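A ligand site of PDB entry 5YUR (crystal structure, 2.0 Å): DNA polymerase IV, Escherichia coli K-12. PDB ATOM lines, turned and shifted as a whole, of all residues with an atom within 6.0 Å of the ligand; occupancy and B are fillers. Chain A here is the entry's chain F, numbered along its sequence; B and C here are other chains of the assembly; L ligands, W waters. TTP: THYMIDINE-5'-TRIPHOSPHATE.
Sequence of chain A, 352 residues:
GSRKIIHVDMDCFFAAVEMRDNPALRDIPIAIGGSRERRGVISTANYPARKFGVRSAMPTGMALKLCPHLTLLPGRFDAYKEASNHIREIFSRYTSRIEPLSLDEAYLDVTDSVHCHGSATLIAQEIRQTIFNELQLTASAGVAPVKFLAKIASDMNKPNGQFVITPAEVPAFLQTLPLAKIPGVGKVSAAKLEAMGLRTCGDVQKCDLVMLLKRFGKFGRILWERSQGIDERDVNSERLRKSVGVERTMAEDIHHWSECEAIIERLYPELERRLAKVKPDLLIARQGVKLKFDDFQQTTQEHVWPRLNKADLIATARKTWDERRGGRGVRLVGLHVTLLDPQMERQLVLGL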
ATOM      1  N   ASP A   9      28.459   7.787 -15.304  1.00  0.00           N
ATOM      2  CA  ASP A   9      27.661   8.113 -14.132  1.00  0.00           C
ATOM      3  C   ASP A   9      27.500   9.621 -14.035  1.00  0.00           C
ATOM      4  O   ASP A   9      28.504  10.310 -13.812  1.00  0.00           O
ATOM      5  CB  ASP A   9      28.350   7.566 -12.864  1.00  0.00           C
ATOM      6  CG  ASP A   9      27.485   7.680 -11.631  1.00  0.00           C
ATOM      7  OD1 ASP A   9      26.797   8.701 -11.523  1.00  0.00           O
ATOM      8  OD2 ASP A   9      27.480   6.772 -10.786  1.00  0.00           O
ATOM      9  N   MET A  10      26.279  10.132 -14.149  1.00  0.00           N
ATOM     10  CA  MET A  10      26.027  11.566 -14.100  1.00  0.00           C
ATOM     11  C   MET A  10      26.339  12.111 -12.707  1.00  0.00           C
ATOM     12  O   MET A  10      26.115  11.417 -11.713  1.00  0.00           O
ATOM     13  CB  MET A  10      24.581  11.898 -14.459  1.00  0.00           C
ATOM     14  CG  MET A  10      24.142  11.502 -15.854  1.00  0.00           C
ATOM     15  SD  MET A  10      25.176  12.208 -17.175  1.00  0.00           S
ATOM     16  CE  MET A  10      24.664  13.910 -17.123  1.00  0.00           C
ATOM     17  N   ASP A  11      26.877  13.340 -12.634  1.00  0.00           N
ATOM     18  CA  ASP A  11      27.185  13.953 -11.336  1.00  0.00           C
ATOM     19  C   ASP A  11      25.931  14.568 -10.719  1.00  0.00           C
ATOM     20  O   ASP A  11      25.211  15.321 -11.383  1.00  0.00           O
ATOM     21  CB  ASP A  11      28.247  15.031 -11.472  1.00  0.00           C
ATOM     22  CG  ASP A  11      29.526  14.535 -12.124  1.00  0.00           C
ATOM     23  OD1 ASP A  11      30.075  13.498 -11.713  1.00  0.00           O
ATOM     24  OD2 ASP A  11      29.947  15.188 -13.085  1.00  0.00           O
ATOM     25  N   CYS A  12      25.695  14.293  -9.430  1.00  0.00           N
ATOM     26  CA  CYS A  12      24.610  14.905  -8.659  1.00  0.00           C
ATOM     27  C   CYS A  12      23.318  15.017  -9.469  1.00  0.00           C
ATOM     28  O   CYS A  12      22.688  16.090  -9.532  1.00  0.00           O
ATOM     29  CB  CYS A  12      25.034  16.278  -8.124  1.00  0.00           C
ATOM     30  SG  CYS A  12      26.422  16.136  -7.016  1.00  0.00           S
ATOM     31  N   PHE A  13      22.908  13.882 -10.058  1.00  0.00           N
ATOM     32  CA  PHE A  13      22.070  13.921 -11.257  1.00  0.00           C
ATOM     33  C   PHE A  13      20.853  14.830 -11.088  1.00  0.00           C
ATOM     34  O   PHE A  13      20.727  15.837 -11.792  1.00  0.00           O
ATOM     35  CB  PHE A  13      21.638  12.504 -11.655  1.00  0.00           C
ATOM     36  CG  PHE A  13      20.802  12.469 -12.894  1.00  0.00           C
ATOM     37  CD1 PHE A  13      21.144  13.208 -14.009  1.00  0.00           C
ATOM     38  CD2 PHE A  13      19.655  11.653 -12.940  1.00  0.00           C
ATOM     39  CE1 PHE A  13      20.366  13.164 -15.157  1.00  0.00           C
ATOM     40  CE2 PHE A  13      18.882  11.588 -14.079  1.00  0.00           C
ATOM     41  CZ  PHE A  13      19.216  12.350 -15.185  1.00  0.00           C
ATOM     42  N   PHE A  14      19.950  14.486 -10.161  1.00  0.00           N
ATOM     43  CA  PHE A  14      18.747  15.301 -10.011  1.00  0.00           C
ATOM     44  C   PHE A  14      19.113  16.754  -9.720  1.00  0.00           C
ATOM     45  O   PHE A  14      18.563  17.679 -10.333  1.00  0.00           O
ATOM     46  CB  PHE A  14      17.845  14.800  -8.865  1.00  0.00           C
ATOM     47  CG  PHE A  14      17.149  13.487  -9.117  1.00  0.00           C
ATOM     48  CD1 PHE A  14      17.407  12.713 -10.236  1.00  0.00           C
ATOM     49  CD2 PHE A  14      16.257  13.025  -8.172  1.00  0.00           C
ATOM     50  CE1 PHE A  14      16.757  11.497 -10.396  1.00  0.00           C
ATOM     51  CE2 PHE A  14      15.590  11.845  -8.320  1.00  0.00           C
ATOM     52  CZ  PHE A  14      15.842  11.064  -9.428  1.00  0.00           C
ATOM     53  N   ALA A  15      20.021  16.972  -8.773  1.00  0.00           N
ATOM     54  CA  ALA A  15      20.381  18.351  -8.429  1.00  0.00           C
ATOM     55  C   ALA A  15      21.055  19.064  -9.599  1.00  0.00           C
ATOM     56  O   ALA A  15      20.744  20.235  -9.869  1.00  0.00           O
ATOM     57  CB  ALA A  15      21.283  18.377  -7.191  1.00  0.00           C
ATOM     58  N   ILE A  42      16.222  12.802   1.683  1.00  0.00           N
ATOM     59  CA  ILE A  42      16.944  13.446   0.586  1.00  0.00           C
ATOM     60  C   ILE A  42      17.140  12.447  -0.528  1.00  0.00           C
ATOM     61  O   ILE A  42      17.686  11.350  -0.300  1.00  0.00           O
ATOM     62  CB  ILE A  42      18.301  13.997   1.078  1.00  0.00           C
ATOM     63  CG1 ILE A  42      18.085  15.069   2.154  1.00  0.00           C
ATOM     64  CG2 ILE A  42      19.125  14.503  -0.109  1.00  0.00           C
ATOM     65  CD1 ILE A  42      17.217  16.188   1.694  1.00  0.00           C
ATOM     66  N   SER A  43      16.723  12.802  -1.751  1.00  0.00           N
ATOM     67  CA  SER A  43      17.089  11.974  -2.902  1.00  0.00           C
ATOM     68  C   SER A  43      18.546  12.213  -3.276  1.00  0.00           C
ATOM     69  O   SER A  43      19.325  11.265  -3.424  1.00  0.00           O
ATOM     70  CB  SER A  43      16.187  12.272  -4.110  1.00  0.00           C
ATOM     71  OG  SER A  43      15.019  11.476  -4.085  1.00  0.00           O
ATOM     72  N   THR A  44      18.903  13.477  -3.468  1.00  0.00           N
ATOM     73  CA  THR A  44      20.296  13.846  -3.634  1.00  0.00           C
ATOM     74  C   THR A  44      20.463  15.342  -3.358  1.00  0.00           C
ATOM     75  O   THR A  44      19.494  16.096  -3.257  1.00  0.00           O
ATOM     76  CB  THR A  44      20.807  13.494  -5.039  1.00  0.00           C
ATOM     77  OG1 THR A  44      22.224  13.644  -5.054  1.00  0.00           O
ATOM     78  CG2 THR A  44      20.209  14.441  -6.053  1.00  0.00           C
ATOM     79  N   ALA A  45      21.723  15.748  -3.278  1.00  0.00           N
ATOM     80  CA  ALA A  45      22.103  17.108  -2.918  1.00  0.00           C
ATOM     81  C   ALA A  45      23.242  17.578  -3.798  1.00  0.00           C
ATOM     82  O   ALA A  45      24.060  16.793  -4.283  1.00  0.00           O
ATOM     83  CB  ALA A  45      22.536  17.176  -1.454  1.00  0.00           C
ATOM     84  N   TYR A  47      26.793  19.971  -4.372  1.00  0.00           N
ATOM     85  CA  TYR A  47      28.031  19.989  -3.575  1.00  0.00           C
ATOM     86  C   TYR A  47      27.980  21.053  -2.463  1.00  0.00           C
ATOM     87  O   TYR A  47      28.416  20.769  -1.331  1.00  0.00           O
ATOM     88  CB  TYR A  47      29.242  20.182  -4.497  1.00  0.00           C
ATOM     89  CG  TYR A  47      29.692  18.849  -5.035  1.00  0.00           C
ATOM     90  CD1 TYR A  47      30.373  17.957  -4.230  1.00  0.00           C
ATOM     91  CD2 TYR A  47      29.336  18.441  -6.312  1.00  0.00           C
ATOM     92  CE1 TYR A  47      30.728  16.690  -4.689  1.00  0.00           C
ATOM     93  CE2 TYR A  47      29.685  17.172  -6.783  1.00  0.00           C
ATOM     94  CZ  TYR A  47      30.377  16.312  -5.955  1.00  0.00           C
ATOM     95  OH  TYR A  47      30.746  15.060  -6.407  1.00  0.00           O
ATOM     96  N   ARG A  50      26.267  19.021   0.155  1.00  0.00           N
ATOM     97  CA  ARG A  50      27.100  17.923   0.637  1.00  0.00           C
ATOM     98  C   ARG A  50      28.214  18.436   1.554  1.00  0.00           C
ATOM     99  O   ARG A  50      28.638  17.742   2.497  1.00  0.00           O
ATOM    100  CB  ARG A  50      27.744  17.140  -0.518  1.00  0.00           C
ATOM    101  CG  ARG A  50      26.744  16.612  -1.522  1.00  0.00           C
ATOM    102  CD  ARG A  50      27.365  15.718  -2.635  1.00  0.00           C
ATOM    103  NE  ARG A  50      26.277  15.180  -3.458  1.00  0.00           N
ATOM    104  CZ  ARG A  50      26.412  14.277  -4.426  1.00  0.00           C
ATOM    105  NH1 ARG A  50      27.594  13.788  -4.718  1.00  0.00           N
ATOM    106  NH2 ARG A  50      25.338  13.889  -5.107  1.00  0.00           N
ATOM    107  N   SER A  56      22.345  11.620   0.031  1.00  0.00           N
ATOM    108  CA  SER A  56      21.210  10.784  -0.386  1.00  0.00           C
ATOM    109  C   SER A  56      20.833   9.844   0.741  1.00  0.00           C
ATOM    110  O   SER A  56      21.695   9.318   1.447  1.00  0.00           O
ATOM    111  CB  SER A  56      21.573   9.947  -1.630  1.00  0.00           C
ATOM    112  OG  SER A  56      21.855  10.752  -2.772  1.00  0.00           O
ATOM    113  N   ALA A  57      19.522   9.640   0.940  1.00  0.00           N
ATOM    114  CA  ALA A  57      18.935   8.704   1.878  1.00  0.00           C
ATOM    115  C   ALA A  57      18.903   9.259   3.301  1.00  0.00           C
ATOM    116  O   ALA A  57      18.393   8.594   4.197  1.00  0.00           O
ATOM    117  CB  ALA A  57      19.632   7.330   1.866  1.00  0.00           C
ATOM    118  N   SER A 102      19.861   2.545 -14.391  1.00  0.00           N
ATOM    119  CA  SER A 102      19.083   3.577 -13.734  1.00  0.00           C
ATOM    120  C   SER A 102      18.999   4.746 -14.703  1.00  0.00           C
ATOM    121  O   SER A 102      19.583   4.671 -15.782  1.00  0.00           O
ATOM    122  CB  SER A 102      19.697   3.986 -12.390  1.00  0.00           C
ATOM    123  OG  SER A 102      21.011   4.545 -12.532  1.00  0.00           O
ATOM    124  N   ASP A 104      20.538   7.510 -14.699  1.00  0.00           N
ATOM    125  CA  ASP A 104      21.722   8.351 -14.866  1.00  0.00           C
ATOM    126  C   ASP A 104      23.018   7.571 -15.076  1.00  0.00           C
ATOM    127  O   ASP A 104      24.105   8.175 -15.044  1.00  0.00           O
ATOM    128  CB  ASP A 104      21.872   9.286 -13.672  1.00  0.00           C
ATOM    129  CG  ASP A 104      22.661   8.670 -12.518  1.00  0.00           C
ATOM    130  OD1 ASP A 104      22.528   7.452 -12.215  1.00  0.00           O
ATOM    131  OD2 ASP A 104      23.441   9.447 -11.896  1.00  0.00           O
ATOM    132  N   GLU A 105      22.941   6.278 -15.303  1.00  0.00           N
ATOM    133  CA  GLU A 105      24.186   5.538 -15.435  1.00  0.00           C
ATOM    134  C   GLU A 105      23.990   4.329 -16.332  1.00  0.00           C
ATOM    135  O   GLU A 105      22.889   3.830 -16.521  1.00  0.00           O
ATOM    136  CB  GLU A 105      24.785   5.209 -14.053  1.00  0.00           C
ATOM    137  CG  GLU A 105      24.091   4.221 -13.150  1.00  0.00           C
ATOM    138  CD  GLU A 105      24.819   4.107 -11.773  1.00  0.00           C
ATOM    139  OE1 GLU A 105      24.788   5.066 -10.953  1.00  0.00           O
ATOM    140  OE2 GLU A 105      25.404   3.036 -11.512  1.00  0.00           O
ATOM    141  N   ASP A 155      33.411   6.440  -9.541  1.00  0.00           N
ATOM    142  CA  ASP A 155      33.235   7.249  -8.348  1.00  0.00           C
ATOM    143  C   ASP A 155      34.509   7.940  -7.904  1.00  0.00           C
ATOM    144  O   ASP A 155      34.445   8.816  -7.040  1.00  0.00           O
ATOM    145  CB  ASP A 155      32.754   6.392  -7.179  1.00  0.00           C
ATOM    146  CG  ASP A 155      31.280   6.155  -7.212  1.00  0.00           C
ATOM    147  OD1 ASP A 155      30.565   6.970  -7.822  1.00  0.00           O
ATOM    148  OD2 ASP A 155      30.852   5.146  -6.626  1.00  0.00           O
ATOM    149  N   LYS A 158      35.203  11.878  -9.215  1.00  0.00           N
ATOM    150  CA  LYS A 158      33.933  12.582  -9.288  1.00  0.00           C
ATOM    151  C   LYS A 158      34.076  13.883  -8.513  1.00  0.00           C
ATOM    152  O   LYS A 158      34.626  13.842  -7.438  1.00  0.00           O
ATOM    153  CB  LYS A 158      32.812  11.763  -8.645  1.00  0.00           C
ATOM    154  CG  LYS A 158      31.912  11.014  -9.568  1.00  0.00           C
ATOM    155  CD  LYS A 158      30.629  10.658  -8.813  1.00  0.00           C
ATOM    156  CE  LYS A 158      29.700   9.886  -9.726  1.00  0.00           C
ATOM    157  NZ  LYS A 158      29.072  10.743 -10.778  1.00  0.00           N
ATOM    158  P    DA B   4      11.152   6.801   5.017  1.00  0.00           P
ATOM    159  OP1  DA B   4       9.849   6.882   5.743  1.00  0.00           O
ATOM    160  OP2  DA B   4      11.747   5.452   4.894  1.00  0.00           O
ATOM    161  O5'  DA B   4      11.023   7.513   3.618  1.00  0.00           O
ATOM    162  C5'  DA B   4      10.423   8.770   3.532  1.00  0.00           C
ATOM    163  C4'  DA B   4       9.918   9.038   2.133  1.00  0.00           C
ATOM    164  O4'  DA B   4      11.036   9.118   1.202  1.00  0.00           O
ATOM    165  C3'  DA B   4       8.986   7.959   1.580  1.00  0.00           C
ATOM    166  O3'  DA B   4       8.015   8.557   0.793  1.00  0.00           O
ATOM    167  C2'  DA B   4       9.923   7.060   0.730  1.00  0.00           C
ATOM    168  C1'  DA B   4      11.043   8.015   0.309  1.00  0.00           C
ATOM    169  N9   DA B   4      12.375   7.425   0.352  1.00  0.00           N
ATOM    170  C8   DA B   4      12.875   6.580   1.308  1.00  0.00           C
ATOM    171  N7   DA B   4      14.139   6.248   1.113  1.00  0.00           N
ATOM    172  C5   DA B   4      14.488   6.943  -0.032  1.00  0.00           C
ATOM    173  C6   DA B   4      15.709   7.010  -0.783  1.00  0.00           C
ATOM    174  N6   DA B   4      16.817   6.358  -0.434  1.00  0.00           N
ATOM    175  N1   DA B   4      15.722   7.802  -1.881  1.00  0.00           N
ATOM    176  C2   DA B   4      14.600   8.448  -2.214  1.00  0.00           C
ATOM    177  N3   DA B   4      13.391   8.454  -1.591  1.00  0.00           N
ATOM    178  C4   DA B   4      13.416   7.671  -0.505  1.00  0.00           C
ATOM    179  P    DG B   5       6.851   7.636   0.185  1.00  0.00           P
ATOM    180  OP1  DG B   5       5.721   8.541  -0.113  1.00  0.00           O
ATOM    181  OP2  DG B   5       6.822   6.431   1.065  1.00  0.00           O
ATOM    182  O5'  DG B   5       7.426   7.202  -1.227  1.00  0.00           O
ATOM    183  C5'  DG B   5       7.520   8.165  -2.228  1.00  0.00           C
ATOM    184  C4'  DG B   5       8.100   7.539  -3.482  1.00  0.00           C
ATOM    185  O4'  DG B   5       9.484   7.205  -3.266  1.00  0.00           O
ATOM    186  C3'  DG B   5       7.411   6.252  -3.917  1.00  0.00           C
ATOM    187  O3'  DG B   5       7.250   6.279  -5.308  1.00  0.00           O
ATOM    188  C2'  DG B   5       8.387   5.165  -3.485  1.00  0.00           C
ATOM    189  C1'  DG B   5       9.707   5.884  -3.675  1.00  0.00           C
ATOM    190  N9   DG B   5      10.807   5.305  -2.923  1.00  0.00           N
ATOM    191  C8   DG B   5      10.751   4.650  -1.709  1.00  0.00           C
ATOM    192  N7   DG B   5      11.926   4.229  -1.288  1.00  0.00           N
ATOM    193  C5   DG B   5      12.802   4.626  -2.312  1.00  0.00           C
ATOM    194  C6   DG B   5      14.219   4.452  -2.445  1.00  0.00           C
ATOM    195  O6   DG B   5      15.012   3.892  -1.675  1.00  0.00           O
ATOM    196  N1   DG B   5      14.692   5.017  -3.613  1.00  0.00           N
ATOM    197  C2   DG B   5      13.936   5.671  -4.549  1.00  0.00           C
ATOM    198  N2   DG B   5      14.600   6.134  -5.633  1.00  0.00           N
ATOM    199  N3   DG B   5      12.632   5.857  -4.435  1.00  0.00           N
ATOM    200  C4   DG B   5      12.130   5.301  -3.301  1.00  0.00           C
ATOM    201  P    DC C  18      23.992   2.050  -7.159  1.00  0.00           P
ATOM    202  OP1  DC C  18      24.705   1.914  -8.448  1.00  0.00           O
ATOM    203  OP2  DC C  18      24.613   2.591  -5.931  1.00  0.00           O
ATOM    204  O5'  DC C  18      22.700   2.888  -7.534  1.00  0.00           O
ATOM    205  C5'  DC C  18      22.020   2.604  -8.717  1.00  0.00           C
ATOM    206  C4'  DC C  18      20.883   3.565  -8.875  1.00  0.00           C
ATOM    207  O4'  DC C  18      19.932   3.346  -7.796  1.00  0.00           O
ATOM    208  C3'  DC C  18      21.300   5.034  -8.812  1.00  0.00           C
ATOM    209  O3'  DC C  18      20.788   5.733  -9.950  1.00  0.00           O
ATOM    210  C2'  DC C  18      20.679   5.535  -7.489  1.00  0.00           C
ATOM    211  C1'  DC C  18      19.508   4.585  -7.298  1.00  0.00           C
ATOM    212  N1   DC C  18      19.116   4.360  -5.895  1.00  0.00           N
ATOM    213  C2   DC C  18      17.885   4.806  -5.501  1.00  0.00           C
ATOM    214  O2   DC C  18      17.199   5.408  -6.346  1.00  0.00           O
ATOM    215  N3   DC C  18      17.483   4.576  -4.228  1.00  0.00           N
ATOM    216  C4   DC C  18      18.276   3.931  -3.376  1.00  0.00           C
ATOM    217  N4   DC C  18      17.840   3.731  -2.146  1.00  0.00           N
ATOM    218  C5   DC C  18      19.577   3.469  -3.764  1.00  0.00           C
ATOM    219  C6   DC C  18      19.937   3.697  -5.031  1.00  0.00           C
HETATM  220  PA  TTP L   1      23.628   8.429  -7.644  1.00  0.00           P
HETATM  221  O1A TTP L   1      23.936   7.421  -6.562  1.00  0.00           O
HETATM  222  O2A TTP L   1      24.455   8.133  -8.890  1.00  0.00           O
HETATM  223  O3A TTP L   1      23.998   9.800  -6.953  1.00  0.00           O
HETATM  224  PB  TTP L   1      24.169  11.267  -7.571  1.00  0.00           P
HETATM  225  O1B TTP L   1      23.152  12.192  -6.987  1.00  0.00           O
HETATM  226  O2B TTP L   1      23.961  11.484  -9.026  1.00  0.00           O
HETATM  227  O3B TTP L   1      25.551  11.654  -6.879  1.00  0.00           O
HETATM  228  PG  TTP L   1      26.984  11.302  -7.468  1.00  0.00           P
HETATM  229  O1G TTP L   1      27.423  12.479  -8.314  1.00  0.00           O
HETATM  230  O2G TTP L   1      26.961  10.059  -8.313  1.00  0.00           O
HETATM  231  O3G TTP L   1      27.805  11.043  -6.241  1.00  0.00           O
HETATM  232  O5' TTP L   1      22.005   8.482  -7.830  1.00  0.00           O
HETATM  233  C5' TTP L   1      21.426   8.925  -9.061  1.00  0.00           C
HETATM  234  C4' TTP L   1      20.141   9.688  -8.743  1.00  0.00           C
HETATM  235  O4' TTP L   1      19.125   8.848  -8.158  1.00  0.00           O
HETATM  236  C3' TTP L   1      20.367  10.810  -7.724  1.00  0.00           C
HETATM  237  O3' TTP L   1      20.662  12.048  -8.367  1.00  0.00           O
HETATM  238  C2' TTP L   1      19.030  10.930  -7.018  1.00  0.00           C
HETATM  239  C1' TTP L   1      18.474   9.511  -7.064  1.00  0.00           C
HETATM  240  N1  TTP L   1      18.737   8.809  -5.799  1.00  0.00           N
HETATM  241  C2  TTP L   1      17.676   8.697  -4.868  1.00  0.00           C
HETATM  242  O2  TTP L   1      16.558   9.191  -5.152  1.00  0.00           O
HETATM  243  N3  TTP L   1      17.828   8.071  -3.708  1.00  0.00           N
HETATM  244  C4  TTP L   1      18.990   7.528  -3.360  1.00  0.00           C
HETATM  245  O4  TTP L   1      19.117   6.946  -2.248  1.00  0.00           O
HETATM  246  C5  TTP L   1      20.128   7.630  -4.296  1.00  0.00           C
HETATM  247  C5M TTP L   1      21.450   7.019  -3.878  1.00  0.00           C
HETATM  248  C6  TTP L   1      19.956   8.292  -5.515  1.00  0.00           C
HETATM  249  O   HOH W   1      16.243   7.004  -8.307  1.00  0.00           O
HETATM  250  O   HOH W   2      24.100  10.091  -3.759  1.00  0.00           O
HETATM  251  O   HOH W   3      26.757  10.310  -3.784  1.00  0.00           O
HETATM  252  O   HOH W   4      19.597   7.991 -11.828  1.00  0.00           O
HETATM  253  O   HOH W   5      20.920   5.269  -1.004  1.00  0.00           O
HETATM  254  O   HOH W   6      26.899   7.575  -8.276  1.00  0.00           O
HETATM  255  O   HOH W   7      26.101   5.303  -7.851  1.00  0.00           O
HETATM  256  O   HOH W   8      29.345  14.240  -8.488  1.00  0.00           O
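Water W6 bridges an oxygen (O2G) of the ligand (2.5 Å) and the side-chain carboxylate of Asp 9 (2.7 Å).
Water W8 lies within hydrogen-bond range of O1G of the ligand (2.6 Å), OH of Tyr 47 (2.6 Å), OD1 of Asp 11 (3.4 Å) and SG of Cys 12 (3.8 Å).
Water W2 lies within hydrogen-bond range of the side-chain hydroxyl (OG) of Ser 56 (2.5 Å) and an oxygen (O3A) of the ligand (3.2 Å).
Water W7 bridges O1A of the ligand (3.3 Å) and OE1 of Glu 105 (3.4 Å).
Water W4 bridges OD1 of Asp 104 and O3' of DC 18 of chain C.
The side-chain carboxylate (OD1) of Asp 9 lies close to an oxygen (O2G) of the ligand (3.5 Å).
O of Met 10 sits close to O2B of the ligand.
The side-chain carboxylate of Asp 104 lies close to an oxygen (O2A) of the ligand.
N4 of DC 18 of chain C lies close to O4 of the ligand, 3.5 Å away.
Residues that only touch the ligand: Asp 11 (3.4 Å), Ser 56 (3.7 Å), Glu 105 (3.7 Å) and DG 5 of chain B (3.7 Å).
Hydrophobic or aromatic side chains that line the ligand: Phe 13 and Phe 14.
Within 4 Å of the ligand: Asp 9, Met 10, Asp 11, Cys 12, Phe 13, Phe 14, Ser 43, Thr 44, Arg 50, Ser 56, Asp 104, Glu 105, Lys 158, DA 4 of chain B, DG 5 of chain B and DC 18 of chain C.
The nearest printed residue that does not touch the ligand is Ala 57 (4.2 Å).
The guanidinium group of Arg 50 lies within hydrogen-bond range of the side-chain hydroxyl of Thr 44 (3.1 Å).
The side-chain sulfur (SG) of Cys 12 lies within hydrogen-bond range of the backbone carbonyl oxygen (O) of Ala 45.
NE of Arg 50 lies within hydrogen-bond range of O of Ala 45, 2.9 Å away.
The backbone carbonyl oxygen (O) of Ser 43 is in hydrogen-bond range of the side-chain hydroxyl (OG) of Ser 56, at 2.7 Å.
NZ of Lys 158 lies within salt-bridge range of OD1 of Asp 11 (3.1 Å).
The side-chain amino group of Lys 158 lies within hydrogen-bond range of the backbone carbonyl oxygen of Met 10, at 3.2 Å.
The side-chain amino group of Lys 158 is in salt-bridge range of the side-chain carboxylate of Asp 9, at 3.1 Å.
The side-chain hydroxyl (OG) of Ser 102 sits at hydrogen-bond distance from the side-chain carboxylate (OD1) of Asp 104, 3.3 Å away.
OG1 of Thr 44 lies within hydrogen-bond range of O1B of the ligand (2.6 Å).
The backbone NH (N) of Cys 12 sits at hydrogen-bond distance from an oxygen (O1G) of the ligand (2.7 Å).
N1 of DA 4 of chain B is in hydrogen-bond range of a nitrogen (N3) of the ligand.
The backbone NH (N) of Phe 13 lies within hydrogen-bond range of an oxygen (O2B) of the ligand (2.8 Å).
An oxygen (O3G) of the ligand lies within salt-bridge range of the guanidinium group of Arg 50, at 3.1 Å.
O2 of the ligand sits at hydrogen-bond distance from OG of Ser 43.
The side-chain amino group (NZ) of Lys 158 lies within salt-bridge range of an oxygen (O2G) of the ligand (3.3 Å).
The backbone NH (N) of Phe 14 sits at hydrogen-bond distance from an oxygen (O3') of the ligand, 3.1 Å away.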
